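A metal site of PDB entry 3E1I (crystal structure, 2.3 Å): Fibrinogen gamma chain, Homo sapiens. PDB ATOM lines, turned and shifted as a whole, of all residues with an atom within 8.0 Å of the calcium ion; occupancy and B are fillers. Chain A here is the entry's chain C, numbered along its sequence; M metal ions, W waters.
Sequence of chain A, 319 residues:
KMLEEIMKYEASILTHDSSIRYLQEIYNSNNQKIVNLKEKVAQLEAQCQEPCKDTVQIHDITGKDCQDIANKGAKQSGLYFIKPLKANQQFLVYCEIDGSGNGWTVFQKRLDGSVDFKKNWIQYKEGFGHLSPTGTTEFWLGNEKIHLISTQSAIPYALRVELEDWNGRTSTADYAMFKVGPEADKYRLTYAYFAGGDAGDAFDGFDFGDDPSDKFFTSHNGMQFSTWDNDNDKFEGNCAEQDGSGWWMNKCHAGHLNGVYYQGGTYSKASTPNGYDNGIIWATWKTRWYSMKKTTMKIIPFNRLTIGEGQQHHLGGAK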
ATOM      1  N   SER A 226     -16.901  15.464  -0.905  1.00  0.00           N
ATOM      2  CA  SER A 226     -16.301  14.290  -1.558  1.00  0.00           C
ATOM      3  C   SER A 226     -14.876  14.025  -1.094  1.00  0.00           C
ATOM      4  O   SER A 226     -14.088  14.947  -0.934  1.00  0.00           O
ATOM      5  CB  SER A 226     -16.285  14.460  -3.095  1.00  0.00           C
ATOM      6  OG  SER A 226     -17.566  14.261  -3.645  1.00  0.00           O
ATOM      7  N   ASN A 230     -15.375   8.276  -1.244  1.00  0.00           N
ATOM      8  CA  ASN A 230     -16.776   8.663  -1.057  1.00  0.00           C
ATOM      9  C   ASN A 230     -17.089   9.816  -2.014  1.00  0.00           C
ATOM     10  O   ASN A 230     -16.968  10.990  -1.672  1.00  0.00           O
ATOM     11  CB  ASN A 230     -17.050   9.059   0.399  1.00  0.00           C
ATOM     12  CG  ASN A 230     -18.500   8.832   0.842  1.00  0.00           C
ATOM     13  OD1 ASN A 230     -18.750   8.187   1.848  1.00  0.00           O
ATOM     14  ND2 ASN A 230     -19.451   9.361   0.084  1.00  0.00           N
ATOM     15  N   ASP A 231     -17.450   9.431  -3.230  1.00  0.00           N
ATOM     16  CA  ASP A 231     -17.628  10.359  -4.340  1.00  0.00           C
ATOM     17  C   ASP A 231     -19.076  10.815  -4.425  1.00  0.00           C
ATOM     18  O   ASP A 231     -19.985  10.033  -4.728  1.00  0.00           O
ATOM     19  CB  ASP A 231     -17.194   9.679  -5.643  1.00  0.00           C
ATOM     20  CG  ASP A 231     -17.438  10.531  -6.881  1.00  0.00           C
ATOM     21  OD1 ASP A 231     -18.231  11.495  -6.826  1.00  0.00           O
ATOM     22  OD2 ASP A 231     -16.830  10.236  -7.923  1.00  0.00           O
ATOM     23  N   ASN A 232     -19.274  12.107  -4.175  1.00  0.00           N
ATOM     24  CA  ASN A 232     -20.607  12.717  -4.159  1.00  0.00           C
ATOM     25  C   ASN A 232     -20.657  13.980  -5.032  1.00  0.00           C
ATOM     26  O   ASN A 232     -21.452  14.889  -4.777  1.00  0.00           O
ATOM     27  CB  ASN A 232     -21.010  13.030  -2.711  1.00  0.00           C
ATOM     28  CG  ASN A 232     -20.865  11.820  -1.782  1.00  0.00           C
ATOM     29  OD1 ASN A 232     -20.021  11.809  -0.883  1.00  0.00           O
ATOM     30  ND2 ASN A 232     -21.666  10.796  -2.029  1.00  0.00           N
ATOM     31  N   ASP A 233     -19.801  14.026  -6.056  1.00  0.00           N
ATOM     32  CA  ASP A 233     -19.694  15.200  -6.923  1.00  0.00           C
ATOM     33  C   ASP A 233     -20.585  15.083  -8.155  1.00  0.00           C
ATOM     34  O   ASP A 233     -21.353  14.109  -8.275  1.00  0.00           O
ATOM     35  CB  ASP A 233     -18.223  15.454  -7.299  1.00  0.00           C
ATOM     36  CG  ASP A 233     -17.650  14.398  -8.240  1.00  0.00           C
ATOM     37  OD1 ASP A 233     -18.413  13.850  -9.074  1.00  0.00           O
ATOM     38  OD2 ASP A 233     -16.434  14.115  -8.160  1.00  0.00           O
ATOM     39  N   LYS A 234     -20.469  16.042  -9.074  1.00  0.00           N
ATOM     40  CA  LYS A 234     -21.318  16.135 -10.282  1.00  0.00           C
ATOM     41  C   LYS A 234     -20.568  15.738 -11.557  1.00  0.00           C
ATOM     42  O   LYS A 234     -20.951  16.141 -12.661  1.00  0.00           O
ATOM     43  CB  LYS A 234     -21.881  17.568 -10.432  1.00  0.00           C
ATOM     44  CG  LYS A 234     -22.731  18.038  -9.243  1.00  0.00           C
ATOM     45  CD  LYS A 234     -24.062  17.320  -9.176  1.00  0.00           C
ATOM     46  CE  LYS A 234     -24.803  17.603  -7.885  1.00  0.00           C
ATOM     47  NZ  LYS A 234     -26.219  17.147  -7.988  1.00  0.00           N
ATOM     48  N   PHE A 235     -19.509  14.961 -11.377  1.00  0.00           N
ATOM     49  CA  PHE A 235     -18.604  14.549 -12.425  1.00  0.00           C
ATOM     50  C   PHE A 235     -18.753  13.033 -12.620  1.00  0.00           C
ATOM     51  O   PHE A 235     -18.972  12.301 -11.653  1.00  0.00           O
ATOM     52  CB  PHE A 235     -17.161  14.910 -12.031  1.00  0.00           C
ATOM     53  CG  PHE A 235     -16.094  14.536 -13.060  1.00  0.00           C
ATOM     54  CD1 PHE A 235     -16.335  14.614 -14.427  1.00  0.00           C
ATOM     55  CD2 PHE A 235     -14.812  14.175 -12.633  1.00  0.00           C
ATOM     56  CE1 PHE A 235     -15.344  14.279 -15.371  1.00  0.00           C
ATOM     57  CE2 PHE A 235     -13.802  13.839 -13.563  1.00  0.00           C
ATOM     58  CZ  PHE A 235     -14.071  13.899 -14.931  1.00  0.00           C
ATOM     59  N   GLU A 236     -18.619  12.596 -13.859  1.00  0.00           N
ATOM     60  CA  GLU A 236     -18.612  11.173 -14.190  1.00  0.00           C
ATOM     61  C   GLU A 236     -17.431  10.459 -13.523  1.00  0.00           C
ATOM     62  O   GLU A 236     -17.573   9.326 -13.070  1.00  0.00           O
ATOM     63  CB  GLU A 236     -18.580  10.998 -15.722  1.00  0.00           C
ATOM     64  CG  GLU A 236     -19.774  11.643 -16.450  1.00  0.00           C
ATOM     65  CD  GLU A 236     -19.945  13.166 -16.193  1.00  0.00           C
ATOM     66  OE1 GLU A 236     -18.962  13.941 -16.280  1.00  0.00           O
ATOM     67  OE2 GLU A 236     -21.094  13.582 -15.890  1.00  0.00           O
ATOM     68  N   GLY A 237     -16.278  11.124 -13.480  1.00  0.00           N
ATOM     69  CA  GLY A 237     -15.110  10.628 -12.754  1.00  0.00           C
ATOM     70  C   GLY A 237     -15.106  11.059 -11.277  1.00  0.00           C
ATOM     71  O   GLY A 237     -16.144  11.402 -10.710  1.00  0.00           O
ATOM     72  N   ASN A 238     -13.907  11.068 -10.686  1.00  0.00           N
ATOM     73  CA  ASN A 238     -13.730  11.263  -9.259  1.00  0.00           C
ATOM     74  C   ASN A 238     -12.846  12.480  -8.981  1.00  0.00           C
ATOM     75  O   ASN A 238     -11.622  12.336  -8.915  1.00  0.00           O
ATOM     76  CB  ASN A 238     -13.105   9.992  -8.642  1.00  0.00           C
ATOM     77  CG  ASN A 238     -13.279   9.904  -7.133  1.00  0.00           C
ATOM     78  OD1 ASN A 238     -13.491   8.805  -6.588  1.00  0.00           O
ATOM     79  ND2 ASN A 238     -13.164  11.023  -6.446  1.00  0.00           N
ATOM     80  N   CYS A 239     -13.473  13.648  -8.809  1.00  0.00           N
ATOM     81  CA  CYS A 239     -12.760  14.927  -8.647  1.00  0.00           C
ATOM     82  C   CYS A 239     -11.773  14.872  -7.497  1.00  0.00           C
ATOM     83  O   CYS A 239     -10.601  15.224  -7.652  1.00  0.00           O
ATOM     84  CB  CYS A 239     -13.741  16.072  -8.363  1.00  0.00           C
ATOM     85  SG  CYS A 239     -14.826  16.578  -9.701  1.00  0.00           S
ATOM     86  N   ALA A 240     -12.248  14.427  -6.340  1.00  0.00           N
ATOM     87  CA  ALA A 240     -11.446  14.353  -5.131  1.00  0.00           C
ATOM     88  C   ALA A 240     -10.240  13.421  -5.288  1.00  0.00           C
ATOM     89  O   ALA A 240      -9.146  13.761  -4.840  1.00  0.00           O
ATOM     90  CB  ALA A 240     -12.309  13.927  -3.946  1.00  0.00           C
ATOM     91  N   MET A 249     -16.840  19.179  -4.003  1.00  0.00           N
ATOM     92  CA  MET A 249     -16.571  19.152  -5.440  1.00  0.00           C
ATOM     93  C   MET A 249     -17.837  19.223  -6.271  1.00  0.00           C
ATOM     94  O   MET A 249     -18.894  18.679  -5.885  1.00  0.00           O
ATOM     95  CB  MET A 249     -15.821  17.868  -5.818  1.00  0.00           C
ATOM     96  CG  MET A 249     -14.428  17.729  -5.227  1.00  0.00           C
ATOM     97  SD  MET A 249     -13.329  19.035  -5.771  1.00  0.00           S
ATOM     98  CE  MET A 249     -11.737  18.313  -5.378  1.00  0.00           C
ATOM     99  N   ASN A 250     -17.705  19.873  -7.415  1.00  0.00           N
ATOM    100  CA  ASN A 250     -18.782  19.980  -8.382  1.00  0.00           C
ATOM    101  C   ASN A 250     -18.297  19.212  -9.626  1.00  0.00           C
ATOM    102  O   ASN A 250     -18.333  17.977  -9.662  1.00  0.00           O
ATOM    103  CB  ASN A 250     -19.059  21.470  -8.660  1.00  0.00           C
ATOM    104  CG  ASN A 250     -20.368  21.717  -9.449  1.00  0.00           C
ATOM    105  OD1 ASN A 250     -20.944  22.802  -9.354  1.00  0.00           O
ATOM    106  ND2 ASN A 250     -20.809  20.746 -10.243  1.00  0.00           N
ATOM    107  N   LYS A 251     -17.825  19.941 -10.627  1.00  0.00           N
ATOM    108  CA  LYS A 251     -17.177  19.310 -11.771  1.00  0.00           C
ATOM    109  C   LYS A 251     -16.118  20.232 -12.382  1.00  0.00           C
ATOM    110  O   LYS A 251     -16.273  20.660 -13.520  1.00  0.00           O
ATOM    111  CB  LYS A 251     -18.224  18.905 -12.819  1.00  0.00           C
ATOM    112  CG  LYS A 251     -17.663  18.030 -13.945  1.00  0.00           C
ATOM    113  CD  LYS A 251     -18.756  17.333 -14.749  1.00  0.00           C
ATOM    114  CE  LYS A 251     -19.532  18.288 -15.648  1.00  0.00           C
ATOM    115  NZ  LYS A 251     -18.843  18.433 -16.956  1.00  0.00           N
ATOM    116  N   CYS A 252     -15.037  20.552 -11.655  1.00  0.00           N
ATOM    117  CA  CYS A 252     -14.805  20.110 -10.268  1.00  0.00           C
ATOM    118  C   CYS A 252     -14.804  21.259  -9.284  1.00  0.00           C
ATOM    119  O   CYS A 252     -15.516  21.195  -8.285  1.00  0.00           O
ATOM    120  CB  CYS A 252     -13.499  19.299 -10.141  1.00  0.00           C
ATOM    121  SG  CYS A 252     -13.601  17.668 -10.907  1.00  0.00           S
HETATM  122 CA    CA M   1     -18.195  11.528  -9.498  1.00  0.00          CA
HETATM  123  O   HOH W   1     -20.545  11.660  -8.932  1.00  0.00           O
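The calcium ion is bound by the side-chain carboxylate (OD1) of Asp 233, the backbone carbonyl oxygen (O) of Gly 237, the backbone carbonyl oxygen (O) of Phe 235, water W1, the side-chain carboxylate (OD2) of Asp 231 and the side-chain carboxylate (OD1) of Asp 231. The calcium ion has six donor atoms within binding distance.
The backbone NH (N) of Asp 233 lies within hydrogen-bond range of the side-chain hydroxyl (OG) of Ser 226, 3.3 Å away. OD2 of Asp 233 is in hydrogen-bond range of N of Cys 239. SG of Cys 252 is disulfide-bonded to SG of Cys 239, 2.0 Å away.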
